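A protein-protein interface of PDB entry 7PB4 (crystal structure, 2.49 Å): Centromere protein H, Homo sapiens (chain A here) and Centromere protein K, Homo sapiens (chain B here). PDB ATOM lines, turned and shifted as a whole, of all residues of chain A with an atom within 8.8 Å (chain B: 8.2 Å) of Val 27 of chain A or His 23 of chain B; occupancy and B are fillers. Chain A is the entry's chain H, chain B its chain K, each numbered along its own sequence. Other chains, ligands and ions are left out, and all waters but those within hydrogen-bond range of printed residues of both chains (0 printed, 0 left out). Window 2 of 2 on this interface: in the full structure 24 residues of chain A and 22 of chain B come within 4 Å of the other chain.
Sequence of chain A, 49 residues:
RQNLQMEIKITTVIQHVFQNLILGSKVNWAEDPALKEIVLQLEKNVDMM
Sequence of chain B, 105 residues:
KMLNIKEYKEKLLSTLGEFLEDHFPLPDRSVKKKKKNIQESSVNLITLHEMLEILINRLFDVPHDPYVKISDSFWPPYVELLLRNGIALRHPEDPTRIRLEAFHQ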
ATOM      1  N   PHE A  18     -13.386  17.149 -26.592  1.00  0.00           N
ATOM      2  CA  PHE A  18     -13.973  15.838 -26.849  1.00  0.00           C
ATOM      3  C   PHE A  18     -12.966  14.728 -26.582  1.00  0.00           C
ATOM      4  O   PHE A  18     -13.300  13.712 -25.959  1.00  0.00           O
ATOM      5  CB  PHE A  18     -14.481  15.772 -28.290  1.00  0.00           C
ATOM      6  CG  PHE A  18     -15.566  14.753 -28.515  1.00  0.00           C
ATOM      7  CD1 PHE A  18     -15.967  13.900 -27.498  1.00  0.00           C
ATOM      8  CD2 PHE A  18     -16.183  14.648 -29.750  1.00  0.00           C
ATOM      9  CE1 PHE A  18     -16.963  12.965 -27.708  1.00  0.00           C
ATOM     10  CE2 PHE A  18     -17.180  13.714 -29.968  1.00  0.00           C
ATOM     11  CZ  PHE A  18     -17.569  12.871 -28.945  1.00  0.00           C
ATOM     12  N   LEU A  21     -12.412  14.343 -22.822  1.00  0.00           N
ATOM     13  CA  LEU A  21     -13.568  13.734 -22.170  1.00  0.00           C
ATOM     14  C   LEU A  21     -13.650  12.242 -22.469  1.00  0.00           C
ATOM     15  O   LEU A  21     -13.968  11.442 -21.580  1.00  0.00           O
ATOM     16  CB  LEU A  21     -14.850  14.444 -22.602  1.00  0.00           C
ATOM     17  CG  LEU A  21     -15.087  15.804 -21.943  1.00  0.00           C
ATOM     18  CD1 LEU A  21     -16.231  16.544 -22.611  1.00  0.00           C
ATOM     19  CD2 LEU A  21     -15.354  15.632 -20.456  1.00  0.00           C
ATOM     20  N   ILE A  22     -13.367  11.848 -23.714  1.00  0.00           N
ATOM     21  CA  ILE A  22     -13.350  10.428 -24.056  1.00  0.00           C
ATOM     22  C   ILE A  22     -12.278   9.701 -23.255  1.00  0.00           C
ATOM     23  O   ILE A  22     -12.482   8.570 -22.796  1.00  0.00           O
ATOM     24  CB  ILE A  22     -13.150  10.243 -25.573  1.00  0.00           C
ATOM     25  CG1 ILE A  22     -14.361  10.773 -26.340  1.00  0.00           C
ATOM     26  CG2 ILE A  22     -12.915   8.778 -25.912  1.00  0.00           C
ATOM     27  CD1 ILE A  22     -14.211  10.692 -27.842  1.00  0.00           C
ATOM     28  N   LEU A  23     -11.123  10.344 -23.060  1.00  0.00           N
ATOM     29  CA  LEU A  23     -10.068   9.722 -22.265  1.00  0.00           C
ATOM     30  C   LEU A  23     -10.461   9.621 -20.795  1.00  0.00           C
ATOM     31  O   LEU A  23     -10.175   8.613 -20.139  1.00  0.00           O
ATOM     32  CB  LEU A  23      -8.765  10.503 -22.418  1.00  0.00           C
ATOM     33  CG  LEU A  23      -7.675   9.795 -23.220  1.00  0.00           C
ATOM     34  CD1 LEU A  23      -6.448  10.675 -23.329  1.00  0.00           C
ATOM     35  CD2 LEU A  23      -7.327   8.461 -22.579  1.00  0.00           C
ATOM     36  N   GLY A  24     -11.112  10.655 -20.259  1.00  0.00           N
ATOM     37  CA  GLY A  24     -11.499  10.629 -18.860  1.00  0.00           C
ATOM     38  C   GLY A  24     -12.632   9.667 -18.566  1.00  0.00           C
ATOM     39  O   GLY A  24     -12.742   9.161 -17.445  1.00  0.00           O
ATOM     40  N   SER A  25     -13.485   9.400 -19.556  1.00  0.00           N
ATOM     41  CA  SER A  25     -14.599   8.486 -19.336  1.00  0.00           C
ATOM     42  C   SER A  25     -14.159   7.028 -19.296  1.00  0.00           C
ATOM     43  O   SER A  25     -14.919   6.182 -18.810  1.00  0.00           O
ATOM     44  CB  SER A  25     -15.663   8.679 -20.419  1.00  0.00           C
ATOM     45  OG  SER A  25     -15.137   8.418 -21.708  1.00  0.00           O
ATOM     46  N   LYS A  26     -12.956   6.721 -19.787  1.00  0.00           N
ATOM     47  CA  LYS A  26     -12.425   5.355 -19.804  1.00  0.00           C
ATOM     48  C   LYS A  26     -13.352   4.402 -20.557  1.00  0.00           C
ATOM     49  O   LYS A  26     -13.526   3.243 -20.176  1.00  0.00           O
ATOM     50  CB  LYS A  26     -12.158   4.843 -18.387  1.00  0.00           C
ATOM     51  CG  LYS A  26     -11.115   5.639 -17.619  1.00  0.00           C
ATOM     52  CD  LYS A  26     -10.852   5.021 -16.255  1.00  0.00           C
ATOM     53  CE  LYS A  26      -9.797   5.800 -15.487  1.00  0.00           C
ATOM     54  NZ  LYS A  26      -9.510   5.188 -14.160  1.00  0.00           N
ATOM     55  N   VAL A  27     -13.948   4.892 -21.638  1.00  0.00           N
ATOM     56  CA  VAL A  27     -14.887   4.112 -22.433  1.00  0.00           C
ATOM     57  C   VAL A  27     -14.121   3.367 -23.517  1.00  0.00           C
ATOM     58  O   VAL A  27     -13.258   3.944 -24.190  1.00  0.00           O
ATOM     59  CB  VAL A  27     -15.971   5.015 -23.044  1.00  0.00           C
ATOM     60  CG1 VAL A  27     -16.834   4.231 -24.020  1.00  0.00           C
ATOM     61  CG2 VAL A  27     -16.826   5.618 -21.949  1.00  0.00           C
ATOM     62  N   ASN A  28     -14.430   2.081 -23.682  1.00  0.00           N
ATOM     63  CA  ASN A  28     -13.872   1.279 -24.769  1.00  0.00           C
ATOM     64  C   ASN A  28     -14.523   1.746 -26.067  1.00  0.00           C
ATOM     65  O   ASN A  28     -15.452   1.131 -26.597  1.00  0.00           O
ATOM     66  CB  ASN A  28     -14.104  -0.206 -24.518  1.00  0.00           C
ATOM     67  CG  ASN A  28     -13.104  -1.083 -25.243  1.00  0.00           C
ATOM     68  OD1 ASN A  28     -12.527  -0.683 -26.254  1.00  0.00           O
ATOM     69  ND2 ASN A  28     -12.896  -2.291 -24.729  1.00  0.00           N
ATOM     70  N   TRP A  29     -14.018   2.868 -26.587  1.00  0.00           N
ATOM     71  CA  TRP A  29     -14.657   3.535 -27.716  1.00  0.00           C
ATOM     72  C   TRP A  29     -14.599   2.718 -29.000  1.00  0.00           C
ATOM     73  O   TRP A  29     -15.366   2.996 -29.928  1.00  0.00           O
ATOM     74  CB  TRP A  29     -14.021   4.908 -27.940  1.00  0.00           C
ATOM     75  CG  TRP A  29     -12.525   4.893 -27.904  1.00  0.00           C
ATOM     76  CD1 TRP A  29     -11.728   5.126 -26.820  1.00  0.00           C
ATOM     77  CD2 TRP A  29     -11.643   4.629 -29.001  1.00  0.00           C
ATOM     78  NE1 TRP A  29     -10.405   5.025 -27.175  1.00  0.00           N
ATOM     79  CE2 TRP A  29     -10.326   4.721 -28.508  1.00  0.00           C
ATOM     80  CE3 TRP A  29     -11.839   4.326 -30.352  1.00  0.00           C
ATOM     81  CZ2 TRP A  29      -9.211   4.519 -29.319  1.00  0.00           C
ATOM     82  CZ3 TRP A  29     -10.731   4.127 -31.154  1.00  0.00           C
ATOM     83  CH2 TRP A  29      -9.434   4.224 -30.635  1.00  0.00           C
ATOM     84  N   ALA A  30     -13.716   1.721 -29.081  1.00  0.00           N
ATOM     85  CA  ALA A  30     -13.705   0.851 -30.252  1.00  0.00           C
ATOM     86  C   ALA A  30     -14.925  -0.056 -30.304  1.00  0.00           C
ATOM     87  O   ALA A  30     -15.297  -0.512 -31.391  1.00  0.00           O
ATOM     88  CB  ALA A  30     -12.427   0.012 -30.279  1.00  0.00           C
ATOM     89  N   GLU A  31     -15.556  -0.326 -29.159  1.00  0.00           N
ATOM     90  CA  GLU A  31     -16.758  -1.153 -29.149  1.00  0.00           C
ATOM     91  C   GLU A  31     -17.957  -0.402 -29.713  1.00  0.00           C
ATOM     92  O   GLU A  31     -18.822  -1.010 -30.354  1.00  0.00           O
ATOM     93  CB  GLU A  31     -17.051  -1.631 -27.727  1.00  0.00           C
ATOM     94  CG  GLU A  31     -15.848  -2.238 -27.019  1.00  0.00           C
ATOM     95  CD  GLU A  31     -15.524  -3.641 -27.496  1.00  0.00           C
ATOM     96  OE1 GLU A  31     -15.854  -4.605 -26.773  1.00  0.00           O
ATOM     97  OE2 GLU A  31     -14.944  -3.781 -28.594  1.00  0.00           O
ATOM     98  N   ASP A  32     -18.028   0.907 -29.487  1.00  0.00           N
ATOM     99  CA  ASP A  32     -19.089   1.732 -30.046  1.00  0.00           C
ATOM    100  C   ASP A  32     -18.704   2.140 -31.462  1.00  0.00           C
ATOM    101  O   ASP A  32     -17.721   2.868 -31.650  1.00  0.00           O
ATOM    102  CB  ASP A  32     -19.328   2.964 -29.168  1.00  0.00           C
ATOM    103  CG  ASP A  32     -20.540   3.769 -29.599  1.00  0.00           C
ATOM    104  OD1 ASP A  32     -21.284   3.310 -30.490  1.00  0.00           O
ATOM    105  OD2 ASP A  32     -20.750   4.867 -29.040  1.00  0.00           O
ATOM    106  N   LEU A  35     -18.773   6.016 -31.986  1.00  0.00           N
ATOM    107  CA  LEU A  35     -17.679   6.602 -31.219  1.00  0.00           C
ATOM    108  C   LEU A  35     -16.330   6.282 -31.850  1.00  0.00           C
ATOM    109  O   LEU A  35     -15.419   7.115 -31.836  1.00  0.00           O
ATOM    110  CB  LEU A  35     -17.722   6.109 -29.774  1.00  0.00           C
ATOM    111  CG  LEU A  35     -18.051   7.152 -28.707  1.00  0.00           C
ATOM    112  CD1 LEU A  35     -17.988   6.527 -27.321  1.00  0.00           C
ATOM    113  CD2 LEU A  35     -17.104   8.336 -28.813  1.00  0.00           C
ATOM    114  N   LYS A  36     -16.187   5.082 -32.415  1.00  0.00           N
ATOM    115  CA  LYS A  36     -14.925   4.712 -33.046  1.00  0.00           C
ATOM    116  C   LYS A  36     -14.677   5.536 -34.303  1.00  0.00           C
ATOM    117  O   LYS A  36     -13.570   6.044 -34.516  1.00  0.00           O
ATOM    118  CB  LYS A  36     -14.910   3.218 -33.371  1.00  0.00           C
ATOM    119  CG  LYS A  36     -13.614   2.749 -34.014  1.00  0.00           C
ATOM    120  CD  LYS A  36     -13.639   1.260 -34.309  1.00  0.00           C
ATOM    121  CE  LYS A  36     -12.323   0.802 -34.921  1.00  0.00           C
ATOM    122  NZ  LYS A  36     -12.328  -0.655 -35.233  1.00  0.00           N
ATOM    123  N   VAL A  39     -13.817   9.129 -33.149  1.00  0.00           N
ATOM    124  CA  VAL A  39     -12.483   9.271 -32.570  1.00  0.00           C
ATOM    125  C   VAL A  39     -11.443   9.434 -33.671  1.00  0.00           C
ATOM    126  O   VAL A  39     -10.509  10.238 -33.554  1.00  0.00           O
ATOM    127  CB  VAL A  39     -12.169   8.070 -31.657  1.00  0.00           C
ATOM    128  CG1 VAL A  39     -10.670   7.915 -31.460  1.00  0.00           C
ATOM    129  CG2 VAL A  39     -12.866   8.233 -30.314  1.00  0.00           C
ATOM    130  N   THR B  15     -22.294  15.036 -31.926  1.00  0.00           N
ATOM    131  CA  THR B  15     -21.810  13.777 -31.375  1.00  0.00           C
ATOM    132  C   THR B  15     -21.253  13.958 -29.967  1.00  0.00           C
ATOM    133  O   THR B  15     -21.438  13.081 -29.116  1.00  0.00           O
ATOM    134  CB  THR B  15     -20.763  13.170 -32.304  1.00  0.00           C
ATOM    135  OG1 THR B  15     -19.647  14.060 -32.420  1.00  0.00           O
ATOM    136  CG2 THR B  15     -21.364  12.934 -33.684  1.00  0.00           C
ATOM    137  N   LEU B  16     -20.601  15.093 -29.693  1.00  0.00           N
ATOM    138  CA  LEU B  16     -20.118  15.369 -28.344  1.00  0.00           C
ATOM    139  C   LEU B  16     -21.273  15.512 -27.364  1.00  0.00           C
ATOM    140  O   LEU B  16     -21.196  15.022 -26.233  1.00  0.00           O
ATOM    141  CB  LEU B  16     -19.255  16.632 -28.348  1.00  0.00           C
ATOM    142  CG  LEU B  16     -18.963  17.282 -26.992  1.00  0.00           C
ATOM    143  CD1 LEU B  16     -18.123  16.370 -26.109  1.00  0.00           C
ATOM    144  CD2 LEU B  16     -18.286  18.635 -27.169  1.00  0.00           C
ATOM    145  N   GLY B  17     -22.348  16.185 -27.776  1.00  0.00           N
ATOM    146  CA  GLY B  17     -23.505  16.306 -26.905  1.00  0.00           C
ATOM    147  C   GLY B  17     -24.140  14.964 -26.603  1.00  0.00           C
ATOM    148  O   GLY B  17     -24.518  14.685 -25.459  1.00  0.00           O
ATOM    149  N   GLU B  18     -24.254  14.107 -27.622  1.00  0.00           N
ATOM    150  CA  GLU B  18     -24.808  12.777 -27.392  1.00  0.00           C
ATOM    151  C   GLU B  18     -23.911  11.961 -26.467  1.00  0.00           C
ATOM    152  O   GLU B  18     -24.400  11.265 -25.568  1.00  0.00           O
ATOM    153  CB  GLU B  18     -25.022  12.055 -28.723  1.00  0.00           C
ATOM    154  CG  GLU B  18     -26.296  11.221 -28.765  1.00  0.00           C
ATOM    155  CD  GLU B  18     -26.621  10.713 -30.156  1.00  0.00           C
ATOM    156  OE1 GLU B  18     -25.720  10.147 -30.810  1.00  0.00           O
ATOM    157  OE2 GLU B  18     -27.777  10.887 -30.598  1.00  0.00           O
ATOM    158  N   PHE B  19     -22.591  12.052 -26.658  1.00  0.00           N
ATOM    159  CA  PHE B  19     -21.656  11.355 -25.780  1.00  0.00           C
ATOM    160  C   PHE B  19     -21.769  11.853 -24.343  1.00  0.00           C
ATOM    161  O   PHE B  19     -21.726  11.058 -23.396  1.00  0.00           O
ATOM    162  CB  PHE B  19     -20.229  11.527 -26.301  1.00  0.00           C
ATOM    163  CG  PHE B  19     -19.170  10.998 -25.375  1.00  0.00           C
ATOM    164  CD1 PHE B  19     -18.847   9.651 -25.369  1.00  0.00           C
ATOM    165  CD2 PHE B  19     -18.488  11.851 -24.522  1.00  0.00           C
ATOM    166  CE1 PHE B  19     -17.870   9.162 -24.520  1.00  0.00           C
ATOM    167  CE2 PHE B  19     -17.511  11.368 -23.671  1.00  0.00           C
ATOM    168  CZ  PHE B  19     -17.202  10.022 -23.671  1.00  0.00           C
ATOM    169  N   LEU B  20     -21.989  13.130 -24.145  1.00  0.00           N
ATOM    170  CA  LEU B  20     -22.054  13.666 -22.796  1.00  0.00           C
ATOM    171  C   LEU B  20     -23.298  13.200 -22.102  1.00  0.00           C
ATOM    172  O   LEU B  20     -23.247  12.775 -20.976  1.00  0.00           O
ATOM    173  CB  LEU B  20     -21.956  15.175 -22.795  1.00  0.00           C
ATOM    174  CG  LEU B  20     -20.652  15.839 -23.188  1.00  0.00           C
ATOM    175  CD1 LEU B  20     -20.817  17.342 -23.132  1.00  0.00           C
ATOM    176  CD2 LEU B  20     -19.536  15.379 -22.276  1.00  0.00           C
ATOM    177  N   GLU B  21     -24.414  13.246 -22.791  1.00  0.00           N
ATOM    178  CA  GLU B  21     -25.640  12.756 -22.232  1.00  0.00           C
ATOM    179  C   GLU B  21     -25.617  11.252 -21.973  1.00  0.00           C
ATOM    180  O   GLU B  21     -26.250  10.765 -21.059  1.00  0.00           O
ATOM    181  CB  GLU B  21     -26.796  13.098 -23.147  1.00  0.00           C
ATOM    182  CG  GLU B  21     -27.432  14.441 -22.864  1.00  0.00           C
ATOM    183  CD  GLU B  21     -28.789  14.573 -23.518  1.00  0.00           C
ATOM    184  OE1 GLU B  21     -29.130  13.715 -24.355  1.00  0.00           O
ATOM    185  OE2 GLU B  21     -29.516  15.531 -23.197  1.00  0.00           O
ATOM    186  N   ASP B  22     -24.865  10.526 -22.781  1.00  0.00           N
ATOM    187  CA  ASP B  22     -24.806   9.084 -22.578  1.00  0.00           C
ATOM    188  C   ASP B  22     -23.834   8.667 -21.482  1.00  0.00           C
ATOM    189  O   ASP B  22     -24.026   7.609 -20.870  1.00  0.00           O
ATOM    190  CB  ASP B  22     -24.423   8.379 -23.884  1.00  0.00           C
ATOM    191  CG  ASP B  22     -25.539   8.403 -24.911  1.00  0.00           C
ATOM    192  OD1 ASP B  22     -26.613   8.968 -24.614  1.00  0.00           O
ATOM    193  OD2 ASP B  22     -25.344   7.852 -26.014  1.00  0.00           O
ATOM    194  N   HIS B  23     -22.794   9.461 -21.211  1.00  0.00           N
ATOM    195  CA  HIS B  23     -21.755   9.046 -20.279  1.00  0.00           C
ATOM    196  C   HIS B  23     -21.562   9.964 -19.080  1.00  0.00           C
ATOM    197  O   HIS B  23     -20.873   9.567 -18.134  1.00  0.00           O
ATOM    198  CB  HIS B  23     -20.411   8.900 -21.010  1.00  0.00           C
ATOM    199  CG  HIS B  23     -20.368   7.747 -21.960  1.00  0.00           C
ATOM    200  ND1 HIS B  23     -20.615   7.882 -23.310  1.00  0.00           N
ATOM    201  CD2 HIS B  23     -20.121   6.431 -21.755  1.00  0.00           C
ATOM    202  CE1 HIS B  23     -20.513   6.703 -23.895  1.00  0.00           C
ATOM    203  NE2 HIS B  23     -20.214   5.805 -22.974  1.00  0.00           N
ATOM    204  N   PHE B  24     -22.133  11.166 -19.082  1.00  0.00           N
ATOM    205  CA  PHE B  24     -22.036  12.082 -17.942  1.00  0.00           C
ATOM    206  C   PHE B  24     -23.401  12.702 -17.674  1.00  0.00           C
ATOM    207  O   PHE B  24     -23.627  13.888 -17.933  1.00  0.00           O
ATOM    208  CB  PHE B  24     -20.979  13.159 -18.195  1.00  0.00           C
ATOM    209  CG  PHE B  24     -19.595  12.613 -18.399  1.00  0.00           C
ATOM    210  CD1 PHE B  24     -18.885  12.077 -17.338  1.00  0.00           C
ATOM    211  CD2 PHE B  24     -19.001  12.643 -19.650  1.00  0.00           C
ATOM    212  CE1 PHE B  24     -17.609  11.576 -17.521  1.00  0.00           C
ATOM    213  CE2 PHE B  24     -17.726  12.144 -19.840  1.00  0.00           C
ATOM    214  CZ  PHE B  24     -17.028  11.610 -18.773  1.00  0.00           C
ATOM    215  N   PRO B  25     -24.337  11.921 -17.143  1.00  0.00           N
ATOM    216  CA  PRO B  25     -25.672  12.449 -16.862  1.00  0.00           C
ATOM    217  C   PRO B  25     -25.764  13.081 -15.479  1.00  0.00           C
ATOM    218  O   PRO B  25     -24.971  12.805 -14.578  1.00  0.00           O
ATOM    219  CB  PRO B  25     -26.554  11.197 -16.947  1.00  0.00           C
ATOM    220  CG  PRO B  25     -25.665  10.114 -16.432  1.00  0.00           C
ATOM    221  CD  PRO B  25     -24.251  10.479 -16.846  1.00  0.00           C
ATOM    222  N   LEU B  26     -26.762  13.949 -15.333  1.00  0.00           N
ATOM    223  CA  LEU B  26     -27.063  14.543 -14.045  1.00  0.00           C
ATOM    224  C   LEU B  26     -27.589  13.476 -13.087  1.00  0.00           C
ATOM    225  O   LEU B  26     -28.040  12.412 -13.518  1.00  0.00           O
ATOM    226  CB  LEU B  26     -28.084  15.666 -14.208  1.00  0.00           C
ATOM    227  CG  LEU B  26     -27.569  16.960 -14.840  1.00  0.00           C
ATOM    228  CD1 LEU B  26     -28.708  17.947 -15.037  1.00  0.00           C
ATOM    229  CD2 LEU B  26     -26.472  17.568 -13.980  1.00  0.00           C
ATOM    230  N   LEU B  48     -23.793  19.469 -18.096  1.00  0.00           N
ATOM    231  CA  LEU B  48     -22.384  19.650 -18.429  1.00  0.00           C
ATOM    232  C   LEU B  48     -22.223  20.302 -19.794  1.00  0.00           C
ATOM    233  O   LEU B  48     -21.231  21.000 -20.041  1.00  0.00           O
ATOM    234  CB  LEU B  48     -21.659  18.304 -18.386  1.00  0.00           C
ATOM    235  CG  LEU B  48     -20.164  18.287 -18.712  1.00  0.00           C
ATOM    236  CD1 LEU B  48     -19.399  19.225 -17.792  1.00  0.00           C
ATOM    237  CD2 LEU B  48     -19.614  16.872 -18.619  1.00  0.00           C
ATOM    238  N   TYR B  78     -18.854  17.713 -11.834  1.00  0.00           N
ATOM    239  CA  TYR B  78     -18.524  18.167 -13.184  1.00  0.00           C
ATOM    240  C   TYR B  78     -17.284  19.057 -13.185  1.00  0.00           C
ATOM    241  O   TYR B  78     -16.422  18.929 -14.065  1.00  0.00           O
ATOM    242  CB  TYR B  78     -19.711  18.909 -13.800  1.00  0.00           C
ATOM    243  CG  TYR B  78     -20.800  18.003 -14.327  1.00  0.00           C
ATOM    244  CD1 TYR B  78     -20.549  16.661 -14.583  1.00  0.00           C
ATOM    245  CD2 TYR B  78     -22.075  18.492 -14.577  1.00  0.00           C
ATOM    246  CE1 TYR B  78     -21.540  15.830 -15.068  1.00  0.00           C
ATOM    247  CE2 TYR B  78     -23.072  17.667 -15.062  1.00  0.00           C
ATOM    248  CZ  TYR B  78     -22.799  16.338 -15.306  1.00  0.00           C
ATOM    249  OH  TYR B  78     -23.791  15.514 -15.789  1.00  0.00           O
ATOM    250  N   LEU B  81     -14.320  16.896 -12.646  1.00  0.00           N
ATOM    251  CA  LEU B  81     -14.062  16.125 -13.856  1.00  0.00           C
ATOM    252  C   LEU B  81     -13.319  16.964 -14.886  1.00  0.00           C
ATOM    253  O   LEU B  81     -12.338  16.510 -15.487  1.00  0.00           O
ATOM    254  CB  LEU B  81     -15.381  15.609 -14.434  1.00  0.00           C
ATOM    255  CG  LEU B  81     -15.314  14.919 -15.797  1.00  0.00           C
ATOM    256  CD1 LEU B  81     -14.737  13.518 -15.665  1.00  0.00           C
ATOM    257  CD2 LEU B  81     -16.686  14.886 -16.452  1.00  0.00           C
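The backbone carbonyl oxygen (O) of Phe 24 of chain B is in hydrogen-bond range of the side-chain hydroxyl (OH) of Tyr 78 of chain B.
The backbone carbonyl oxygen (O) of Ile 22 of chain A lies within hydrogen-bond range of the side-chain hydroxyl (OG) of Ser 25 of chain A (2.9 Å).
The backbone carbonyl oxygen (O) of Leu 21 of chain A sits at hydrogen-bond distance from the side-chain hydroxyl (OG) of Ser 25 of chain A (3.2 Å).
O of Phe 19 of chain B lies close to ND1 of His 23 of chain B (3.4 Å).
Thr 15 of chain B touches Phe 18 of chain A.
Phe 18 of chain A touches Leu 16 of chain B.
CD2 of Phe 19 of chain B touches CE1 of Phe 18 of chain A, 3.7 Å away.
Leu 16 of chain B touches Leu 21 of chain A.
Leu 20 of chain B touches Leu 21 of chain A (CD2 to CD1, 3.5 Å).
CA of Ile 22 of chain A touches CZ of Phe 19 of chain B (3.9 Å).
Phe 19 of chain B touches Ser 25 of chain A.
Ser 25 of chain A touches Phe 24 of chain B (CB to CZ, 3.6 Å).
Val 27 of chain A touches His 23 of chain B (CG2 to CD2, 3.4 Å).
Leu 35 of chain A touches Phe 19 of chain B.
Of the printed residues of chain B, Leu 21 of chain A touches Leu 16 (3.98 Å) and Leu 20 (3.5 Å).
Printed residues of chain B within 4 Å of Ser 25 of chain A: Phe 19 (3.3 Å) and Phe 24 (3.6 Å).
Of the printed residues of chain B, Leu 35 of chain A touches Phe 19 (3.8 Å).
Lys 36 of chain A touches none of the printed residues of chain B.
Of the printed residues of chain A, Thr 15 of chain B touches Phe 18.
Printed residues of chain A within 4 Å of Leu 20 of chain B: Leu 21.
Printed residues of chain A within 4 Å of His 23 of chain B: Val 27.
Of chain A, only Ser 25 (3.6 Å) comes within 4 Å of Phe 24 of chain B.
The nearest residue of chain B that does not touch Val 27 of chain A is Phe 19 of chain B (4.5 Å).
The nearest residue of chain A that does not touch His 23 of chain B is Leu 35 of chain A (4.3 Å).
The nearest printed residue of chain B that does not touch Phe 18 of chain A is Gly 17 of chain B (5.9 Å).
Printed residues of chain B that touch a printed residue of chain A: Thr 15, Leu 16, Phe 19, Leu 20, His 23 and Phe 24.
Hydrophobic or aromatic side chains of chain B that line the printed part of chain A: Leu 16, Phe 19, Leu 20, His 23 and Phe 24.
Printed residues of chain A that touch a printed residue of chain B: Phe 18, Leu 21, Ile 22, Ser 25, Val 27 and Leu 35.
Hydrophobic or aromatic side chains of chain A that line the printed part of chain B: Phe 18, Leu 21, Ile 22, Val 27 and Leu 35.
Among the printed residues, 10 pairs touch across the chains.
Among the printed residues, no Asp or Glu carboxylate lies within 4 Å of a Lys or Arg side-chain nitrogen of the other chain.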
